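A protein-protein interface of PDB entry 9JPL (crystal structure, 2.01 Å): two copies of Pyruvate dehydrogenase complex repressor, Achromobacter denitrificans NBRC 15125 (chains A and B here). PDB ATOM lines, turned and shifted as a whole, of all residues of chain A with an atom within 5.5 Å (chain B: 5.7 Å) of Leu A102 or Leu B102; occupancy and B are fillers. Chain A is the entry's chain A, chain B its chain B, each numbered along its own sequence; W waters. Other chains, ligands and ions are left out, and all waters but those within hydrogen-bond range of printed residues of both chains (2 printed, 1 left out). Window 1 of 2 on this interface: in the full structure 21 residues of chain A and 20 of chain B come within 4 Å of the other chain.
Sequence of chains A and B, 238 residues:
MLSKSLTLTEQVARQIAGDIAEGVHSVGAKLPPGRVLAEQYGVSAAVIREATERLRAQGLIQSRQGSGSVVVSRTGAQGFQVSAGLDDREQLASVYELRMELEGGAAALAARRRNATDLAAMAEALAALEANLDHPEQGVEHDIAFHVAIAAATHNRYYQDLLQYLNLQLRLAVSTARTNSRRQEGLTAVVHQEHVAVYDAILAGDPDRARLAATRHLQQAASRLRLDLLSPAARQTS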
ATOM      1  N   LEU A  98      20.816 -24.756  17.226  1.00  0.00           N
ATOM      2  CA  LEU A  98      19.449 -24.395  16.867  1.00  0.00           C
ATOM      3  C   LEU A  98      19.241 -24.440  15.354  1.00  0.00           C
ATOM      4  O   LEU A  98      18.206 -24.923  14.878  1.00  0.00           O
ATOM      5  CB  LEU A  98      19.130 -23.008  17.432  1.00  0.00           C
ATOM      6  CG  LEU A  98      17.822 -22.369  16.965  1.00  0.00           C
ATOM      7  CD1 LEU A  98      16.598 -23.183  17.405  1.00  0.00           C
ATOM      8  CD2 LEU A  98      17.748 -20.931  17.466  1.00  0.00           C
ATOM      9  N   ARG A  99      20.212 -23.932  14.586  1.00  0.00           N
ATOM     10  CA  ARG A  99      20.132 -23.982  13.132  1.00  0.00           C
ATOM     11  C   ARG A  99      20.012 -25.414  12.634  1.00  0.00           C
ATOM     12  O   ARG A  99      19.296 -25.684  11.662  1.00  0.00           O
ATOM     13  CB  ARG A  99      21.360 -23.301  12.515  1.00  0.00           C
ATOM     14  CG  ARG A  99      21.319 -21.763  12.590  1.00  0.00           C
ATOM     15  CD  ARG A  99      22.558 -21.135  11.930  1.00  0.00           C
ATOM     16  NE  ARG A  99      22.469 -21.264  10.474  1.00  0.00           N
ATOM     17  CZ  ARG A  99      23.487 -21.071   9.644  1.00  0.00           C
ATOM     18  NH1 ARG A  99      24.689 -20.721  10.126  1.00  0.00           N
ATOM     19  NH2 ARG A  99      23.301 -21.218   8.334  1.00  0.00           N
ATOM     20  N   MET A 100      20.729 -26.347  13.265  1.00  0.00           N
ATOM     21  CA  MET A 100      20.674 -27.728  12.806  1.00  0.00           C
ATOM     22  C   MET A 100      19.252 -28.265  12.867  1.00  0.00           C
ATOM     23  O   MET A 100      18.815 -28.970  11.957  1.00  0.00           O
ATOM     24  CB  MET A 100      21.605 -28.606  13.635  1.00  0.00           C
ATOM     25  CG  MET A 100      23.066 -28.489  13.258  1.00  0.00           C
ATOM     26  SD  MET A 100      24.099 -29.496  14.344  1.00  0.00           S
ATOM     27  CE  MET A 100      23.472 -31.113  13.934  1.00  0.00           C
ATOM     28  N   GLU A 101      18.509 -27.917  13.919  1.00  0.00           N
ATOM     29  CA  GLU A 101      17.136 -28.385  14.049  1.00  0.00           C
ATOM     30  C   GLU A 101      16.198 -27.600  13.137  1.00  0.00           C
ATOM     31  O   GLU A 101      15.415 -28.196  12.384  1.00  0.00           O
ATOM     32  CB  GLU A 101      16.696 -28.291  15.508  1.00  0.00           C
ATOM     33  CG  GLU A 101      17.600 -29.063  16.451  1.00  0.00           C
ATOM     34  CD  GLU A 101      17.580 -30.562  16.211  1.00  0.00           C
ATOM     35  OE1 GLU A 101      16.577 -31.072  15.667  1.00  0.00           O
ATOM     36  OE2 GLU A 101      18.569 -31.233  16.583  1.00  0.00           O
ATOM     37  N   LEU A 102      16.295 -26.266  13.158  1.00  0.00           N
ATOM     38  CA  LEU A 102      15.429 -25.439  12.319  1.00  0.00           C
ATOM     39  C   LEU A 102      15.697 -25.671  10.838  1.00  0.00           C
ATOM     40  O   LEU A 102      14.762 -25.891  10.061  1.00  0.00           O
ATOM     41  CB  LEU A 102      15.622 -23.958  12.638  1.00  0.00           C
ATOM     42  CG  LEU A 102      14.567 -23.205  13.440  1.00  0.00           C
ATOM     43  CD1 LEU A 102      14.967 -21.734  13.579  1.00  0.00           C
ATOM     44  CD2 LEU A 102      13.201 -23.329  12.764  1.00  0.00           C
ATOM     45  N   GLU A 103      16.966 -25.581  10.416  1.00  0.00           N
ATOM     46  CA  GLU A 103      17.283 -25.606   8.991  1.00  0.00           C
ATOM     47  C   GLU A 103      17.263 -27.017   8.423  1.00  0.00           C
ATOM     48  O   GLU A 103      16.952 -27.189   7.244  1.00  0.00           O
ATOM     49  CB  GLU A 103      18.641 -24.940   8.720  1.00  0.00           C
ATOM     50  CG  GLU A 103      18.586 -23.425   8.940  1.00  0.00           C
ATOM     51  CD  GLU A 103      19.913 -22.682   8.676  1.00  0.00           C
ATOM     52  OE1 GLU A 103      20.723 -23.102   7.819  1.00  0.00           O
ATOM     53  OE2 GLU A 103      20.140 -21.657   9.355  1.00  0.00           O
ATOM     54  N   GLY A 104      17.582 -28.036   9.227  1.00  0.00           N
ATOM     55  CA  GLY A 104      17.342 -29.396   8.773  1.00  0.00           C
ATOM     56  C   GLY A 104      15.872 -29.633   8.475  1.00  0.00           C
ATOM     57  O   GLY A 104      15.521 -30.237   7.454  1.00  0.00           O
ATOM     58  N   GLY A 105      14.993 -29.137   9.349  1.00  0.00           N
ATOM     59  CA  GLY A 105      13.565 -29.286   9.105  1.00  0.00           C
ATOM     60  C   GLY A 105      13.092 -28.461   7.921  1.00  0.00           C
ATOM     61  O   GLY A 105      12.273 -28.919   7.124  1.00  0.00           O
ATOM     62  N   ALA A 106      13.613 -27.239   7.780  1.00  0.00           N
ATOM     63  CA  ALA A 106      13.231 -26.390   6.657  1.00  0.00           C
ATOM     64  C   ALA A 106      13.619 -27.020   5.327  1.00  0.00           C
ATOM     65  O   ALA A 106      12.874 -26.922   4.343  1.00  0.00           O
ATOM     66  CB  ALA A 106      13.883 -25.016   6.788  1.00  0.00           C
ATOM     67  N   ALA A 107      14.797 -27.646   5.267  1.00  0.00           N
ATOM     68  CA  ALA A 107      15.236 -28.241   4.010  1.00  0.00           C
ATOM     69  C   ALA A 107      14.357 -29.423   3.627  1.00  0.00           C
ATOM     70  O   ALA A 107      14.083 -29.639   2.437  1.00  0.00           O
ATOM     71  CB  ALA A 107      16.695 -28.672   4.118  1.00  0.00           C
ATOM     72  N   TYR A 159       8.182 -20.531   9.697  1.00  0.00           N
ATOM     73  CA  TYR A 159       9.588 -20.833   9.422  1.00  0.00           C
ATOM     74  C   TYR A 159      10.334 -19.607   8.919  1.00  0.00           C
ATOM     75  O   TYR A 159      11.443 -19.305   9.373  1.00  0.00           O
ATOM     76  CB  TYR A 159       9.690 -21.946   8.377  1.00  0.00           C
ATOM     77  CG  TYR A 159      10.100 -23.268   8.948  1.00  0.00           C
ATOM     78  CD1 TYR A 159      11.424 -23.523   9.252  1.00  0.00           C
ATOM     79  CD2 TYR A 159       9.164 -24.252   9.210  1.00  0.00           C
ATOM     80  CE1 TYR A 159      11.808 -24.729   9.779  1.00  0.00           C
ATOM     81  CE2 TYR A 159       9.542 -25.467   9.737  1.00  0.00           C
ATOM     82  CZ  TYR A 159      10.871 -25.688  10.006  1.00  0.00           C
ATOM     83  OH  TYR A 159      11.287 -26.869  10.537  1.00  0.00           O
ATOM     84  N   LEU A 162      10.801 -16.935  11.627  1.00  0.00           N
ATOM     85  CA  LEU A 162      11.823 -17.291  12.603  1.00  0.00           C
ATOM     86  C   LEU A 162      13.233 -16.997  12.093  1.00  0.00           C
ATOM     87  O   LEU A 162      14.088 -16.534  12.856  1.00  0.00           O
ATOM     88  CB  LEU A 162      11.682 -18.761  12.969  1.00  0.00           C
ATOM     89  CG  LEU A 162      10.617 -19.079  14.019  1.00  0.00           C
ATOM     90  CD1 LEU A 162      10.707 -20.556  14.388  1.00  0.00           C
ATOM     91  CD2 LEU A 162      10.785 -18.190  15.250  1.00  0.00           C
ATOM     92  N   LEU A 163      13.509 -17.266  10.810  1.00  0.00           N
ATOM     93  CA  LEU A 163      14.852 -16.988  10.297  1.00  0.00           C
ATOM     94  C   LEU A 163      15.126 -15.488  10.214  1.00  0.00           C
ATOM     95  O   LEU A 163      16.264 -15.045  10.424  1.00  0.00           O
ATOM     96  CB  LEU A 163      15.050 -17.640   8.938  1.00  0.00           C
ATOM     97  CG  LEU A 163      15.922 -18.881   9.055  1.00  0.00           C
ATOM     98  CD1 LEU A 163      15.078 -19.978   9.654  1.00  0.00           C
ATOM     99  CD2 LEU A 163      16.452 -19.294   7.685  1.00  0.00           C
ATOM    100  N   LEU A 166      16.023 -14.288  13.625  1.00  0.00           N
ATOM    101  CA  LEU A 166      17.380 -14.666  14.001  1.00  0.00           C
ATOM    102  C   LEU A 166      18.436 -14.040  13.102  1.00  0.00           C
ATOM    103  O   LEU A 166      19.561 -14.541  13.049  1.00  0.00           O
ATOM    104  CB  LEU A 166      17.524 -16.192  13.971  1.00  0.00           C
ATOM    105  CG  LEU A 166      16.685 -16.984  14.979  1.00  0.00           C
ATOM    106  CD1 LEU A 166      16.651 -18.467  14.608  1.00  0.00           C
ATOM    107  CD2 LEU A 166      17.216 -16.776  16.402  1.00  0.00           C
ATOM    108  N   LEU B  98       5.890 -26.857  12.592  1.00  0.00           N
ATOM    109  CA  LEU B  98       7.055 -26.135  13.089  1.00  0.00           C
ATOM    110  C   LEU B  98       7.456 -26.622  14.479  1.00  0.00           C
ATOM    111  O   LEU B  98       8.650 -26.825  14.750  1.00  0.00           O
ATOM    112  CB  LEU B  98       6.773 -24.637  13.106  1.00  0.00           C
ATOM    113  CG  LEU B  98       7.813 -23.823  13.893  1.00  0.00           C
ATOM    114  CD1 LEU B  98       9.186 -23.859  13.228  1.00  0.00           C
ATOM    115  CD2 LEU B  98       7.349 -22.385  14.091  1.00  0.00           C
ATOM    116  N   ARG B  99       6.473 -26.838  15.363  1.00  0.00           N
ATOM    117  CA  ARG B  99       6.766 -27.367  16.696  1.00  0.00           C
ATOM    118  C   ARG B  99       7.485 -28.702  16.623  1.00  0.00           C
ATOM    119  O   ARG B  99       8.315 -29.004  17.485  1.00  0.00           O
ATOM    120  CB  ARG B  99       5.475 -27.523  17.507  1.00  0.00           C
ATOM    121  CG  ARG B  99       4.840 -26.218  17.910  1.00  0.00           C
ATOM    122  CD  ARG B  99       3.616 -26.460  18.778  1.00  0.00           C
ATOM    123  NE  ARG B  99       3.978 -27.085  20.040  1.00  0.00           N
ATOM    124  CZ  ARG B  99       3.112 -27.671  20.863  1.00  0.00           C
ATOM    125  NH1 ARG B  99       1.818 -27.728  20.546  1.00  0.00           N
ATOM    126  NH2 ARG B  99       3.540 -28.212  21.999  1.00  0.00           N
ATOM    127  N   MET B 100       7.190 -29.504  15.601  1.00  0.00           N
ATOM    128  CA  MET B 100       7.799 -30.824  15.481  1.00  0.00           C
ATOM    129  C   MET B 100       9.308 -30.733  15.301  1.00  0.00           C
ATOM    130  O   MET B 100      10.060 -31.558  15.837  1.00  0.00           O
ATOM    131  CB  MET B 100       7.178 -31.577  14.306  1.00  0.00           C
ATOM    132  CG  MET B 100       6.938 -33.053  14.563  1.00  0.00           C
ATOM    133  SD  MET B 100       5.835 -33.683  13.298  1.00  0.00           S
ATOM    134  CE  MET B 100       4.493 -32.530  13.496  1.00  0.00           C
ATOM    135  N   GLU B 101       9.773 -29.750  14.539  1.00  0.00           N
ATOM    136  CA  GLU B 101      11.212 -29.593  14.363  1.00  0.00           C
ATOM    137  C   GLU B 101      11.863 -28.909  15.564  1.00  0.00           C
ATOM    138  O   GLU B 101      12.984 -29.258  15.951  1.00  0.00           O
ATOM    139  CB  GLU B 101      11.472 -28.826  13.069  1.00  0.00           C
ATOM    140  CG  GLU B 101      10.793 -29.477  11.863  1.00  0.00           C
ATOM    141  CD  GLU B 101      11.472 -30.772  11.428  1.00  0.00           C
ATOM    142  OE1 GLU B 101      12.542 -31.124  11.971  1.00  0.00           O
ATOM    143  OE2 GLU B 101      10.952 -31.425  10.509  1.00  0.00           O
ATOM    144  N   LEU B 102      11.168 -27.957  16.185  1.00  0.00           N
ATOM    145  CA  LEU B 102      11.750 -27.220  17.302  1.00  0.00           C
ATOM    146  C   LEU B 102      11.751 -28.057  18.579  1.00  0.00           C
ATOM    147  O   LEU B 102      12.738 -28.074  19.324  1.00  0.00           O
ATOM    148  CB  LEU B 102      10.967 -25.927  17.539  1.00  0.00           C
ATOM    149  CG  LEU B 102      11.562 -24.575  17.170  1.00  0.00           C
ATOM    150  CD1 LEU B 102      11.816 -24.562  15.698  1.00  0.00           C
ATOM    151  CD2 LEU B 102      10.601 -23.459  17.567  1.00  0.00           C
ATOM    152  N   GLU B 103      10.629 -28.721  18.870  1.00  0.00           N
ATOM    153  CA  GLU B 103      10.480 -29.379  20.162  1.00  0.00           C
ATOM    154  C   GLU B 103      11.139 -30.749  20.178  1.00  0.00           C
ATOM    155  O   GLU B 103      11.619 -31.175  21.233  1.00  0.00           O
ATOM    156  CB  GLU B 103       8.994 -29.451  20.553  1.00  0.00           C
ATOM    157  CG  GLU B 103       8.509 -28.107  21.142  1.00  0.00           C
ATOM    158  CD  GLU B 103       6.983 -27.974  21.273  1.00  0.00           C
ATOM    159  OE1 GLU B 103       6.288 -29.002  21.445  1.00  0.00           O
ATOM    160  OE2 GLU B 103       6.482 -26.823  21.206  1.00  0.00           O
ATOM    161  N   GLY B 104      11.185 -31.445  19.036  1.00  0.00           N
ATOM    162  CA  GLY B 104      12.020 -32.633  18.946  1.00  0.00           C
ATOM    163  C   GLY B 104      13.486 -32.323  19.204  1.00  0.00           C
ATOM    164  O   GLY B 104      14.166 -33.025  19.964  1.00  0.00           O
ATOM    165  N   GLY B 105      13.986 -31.252  18.588  1.00  0.00           N
ATOM    166  CA  GLY B 105      15.346 -30.815  18.876  1.00  0.00           C
ATOM    167  C   GLY B 105      15.549 -30.393  20.322  1.00  0.00           C
ATOM    168  O   GLY B 105      16.590 -30.680  20.919  1.00  0.00           O
ATOM    169  N   ALA B 106      14.565 -29.702  20.911  1.00  0.00           N
ATOM    170  CA  ALA B 106      14.733 -29.253  22.295  1.00  0.00           C
ATOM    171  C   ALA B 106      14.755 -30.432  23.258  1.00  0.00           C
ATOM    172  O   ALA B 106      15.581 -30.480  24.172  1.00  0.00           O
ATOM    173  CB  ALA B 106      13.633 -28.265  22.680  1.00  0.00           C
ATOM    174  N   ALA B 107      13.865 -31.402  23.062  1.00  0.00           N
ATOM    175  CA  ALA B 107      13.869 -32.585  23.913  1.00  0.00           C
ATOM    176  C   ALA B 107      15.206 -33.313  23.854  1.00  0.00           C
ATOM    177  O   ALA B 107      15.707 -33.784  24.883  1.00  0.00           O
ATOM    178  CB  ALA B 107      12.720 -33.522  23.512  1.00  0.00           C
ATOM    179  N   TYR B 159      16.743 -21.256  21.899  1.00  0.00           N
ATOM    180  CA  TYR B 159      15.543 -22.088  21.949  1.00  0.00           C
ATOM    181  C   TYR B 159      14.486 -21.450  22.819  1.00  0.00           C
ATOM    182  O   TYR B 159      13.305 -21.406  22.456  1.00  0.00           O
ATOM    183  CB  TYR B 159      15.856 -23.465  22.510  1.00  0.00           C
ATOM    184  CG  TYR B 159      16.166 -24.494  21.485  1.00  0.00           C
ATOM    185  CD1 TYR B 159      15.155 -25.179  20.809  1.00  0.00           C
ATOM    186  CD2 TYR B 159      17.477 -24.788  21.201  1.00  0.00           C
ATOM    187  CE1 TYR B 159      15.471 -26.135  19.873  1.00  0.00           C
ATOM    188  CE2 TYR B 159      17.799 -25.718  20.288  1.00  0.00           C
ATOM    189  CZ  TYR B 159      16.812 -26.391  19.635  1.00  0.00           C
ATOM    190  OH  TYR B 159      17.227 -27.313  18.742  1.00  0.00           O
ATOM    191  N   LEU B 162      12.912 -18.425  21.143  1.00  0.00           N
ATOM    192  CA  LEU B 162      12.035 -18.772  20.025  1.00  0.00           C
ATOM    193  C   LEU B 162      10.652 -19.206  20.501  1.00  0.00           C
ATOM    194  O   LEU B 162       9.637 -18.859  19.876  1.00  0.00           O
ATOM    195  CB  LEU B 162      12.680 -19.869  19.185  1.00  0.00           C
ATOM    196  CG  LEU B 162      13.410 -19.379  17.940  1.00  0.00           C
ATOM    197  CD1 LEU B 162      14.311 -18.215  18.278  1.00  0.00           C
ATOM    198  CD2 LEU B 162      14.188 -20.526  17.340  1.00  0.00           C
ATOM    199  N   LEU B 163      10.590 -19.971  21.599  1.00  0.00           N
ATOM    200  CA  LEU B 163       9.305 -20.439  22.114  1.00  0.00           C
ATOM    201  C   LEU B 163       8.522 -19.301  22.738  1.00  0.00           C
ATOM    202  O   LEU B 163       7.286 -19.273  22.658  1.00  0.00           O
ATOM    203  CB  LEU B 163       9.509 -21.547  23.145  1.00  0.00           C
ATOM    204  CG  LEU B 163       9.225 -22.957  22.651  1.00  0.00           C
ATOM    205  CD1 LEU B 163      10.329 -23.396  21.710  1.00  0.00           C
ATOM    206  CD2 LEU B 163       9.077 -23.915  23.832  1.00  0.00           C
ATOM    207  N   LEU B 166       7.055 -17.354  19.841  1.00  0.00           N
ATOM    208  CA  LEU B 166       5.930 -18.076  19.274  1.00  0.00           C
ATOM    209  C   LEU B 166       4.832 -18.335  20.291  1.00  0.00           C
ATOM    210  O   LEU B 166       3.992 -19.203  20.058  1.00  0.00           O
ATOM    211  CB  LEU B 166       6.410 -19.406  18.688  1.00  0.00           C
ATOM    212  CG  LEU B 166       7.348 -19.305  17.481  1.00  0.00           C
ATOM    213  CD1 LEU B 166       8.194 -20.565  17.353  1.00  0.00           C
ATOM    214  CD2 LEU B 166       6.551 -19.048  16.217  1.00  0.00           C
HETATM  215  O   HOH W   1      19.004 -31.022  19.177  1.00  0.00           O
HETATM  216  O   HOH W   2      14.489 -30.865  13.827  1.00  0.00           O
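Leu A98 touches Tyr B159. CD2 of Leu B162 touches CD2 of Leu A98, at 3.6 Å. Glu B101 touches Glu A101 (O to CB, 3.9 Å). Glu A101 touches Tyr B159 (CG to OH, 2.9 Å). Leu A102 touches Leu B102. Tyr A159 touches Glu B101. Leu A162 touches Leu B98 (CD1 to CD1, 3.8 Å). CG of Leu B162 touches CD2 of Leu A162 (3.9 Å). Leu A162 touches Leu B166. Leu A166 touches Leu B162 (CD2 to CD1, 3.7 Å).
Printed residues of chain B within 4 Å of Leu A98: Tyr B159 (3.9 Å) and Leu B162 (3.6 Å). Leu A102 touches just one residue of chain B: Leu B102. Of the printed residues of chain B, Gly A105 touches Glu B101 (3.5 Å). Of the printed residues of chain A, Glu B101 touches Glu A101, Gly A105 and Tyr A159. Leu B102 touches one residue of chain A. Printed residues of chain A within 4 Å of Leu B166: Leu A162. The nearest residue of chain B that does not touch Leu A102 is Leu B162 (4.03 Å).
Hydrophobic or aromatic side chains of chain A within 4 Å of the printed part of chain B: Leu A98, Leu A102, Tyr A159, Leu A162 and Leu A166. Printed residues of chain B that touch a printed residue of chain A: Leu B98, Glu B101, Leu B102, Gly B105, Tyr B159, Leu B162 and Leu B166. Hydrophobic or aromatic side chains of chain B within 4 Å of the printed part of chain A: Leu B98, Leu B102, Tyr B159, Leu B162 and Leu B166. Among the printed residues, 13 pairs touch across the chains.
Leu A98 touches Tyr B159, and with the chains exchanged Tyr A159 touches Leu B98. Glu A101 touches Gly B105, and with the chains exchanged Gly A105 touches Glu B101. Glu A101 touches Tyr B159, and with the chains exchanged Tyr A159 touches Glu B101. Leu B102 touches its own counterpart, Leu A102. Positions printed for both chains: 98, 99, 100, 101, 102, 103, 104, 105, 106, 107, 159, 162, 163 and 166.
Water W1 bridges the side-chain carboxylate (OE2) of Glu A101 (2.6 Å) and the backbone carbonyl oxygen (O) of Gly B105 (3.0 Å). Water W2 bridges the side-chain carboxylate of Glu B101 (2.7 Å) and the side-chain carboxylate of Glu A101 (2.8 Å).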
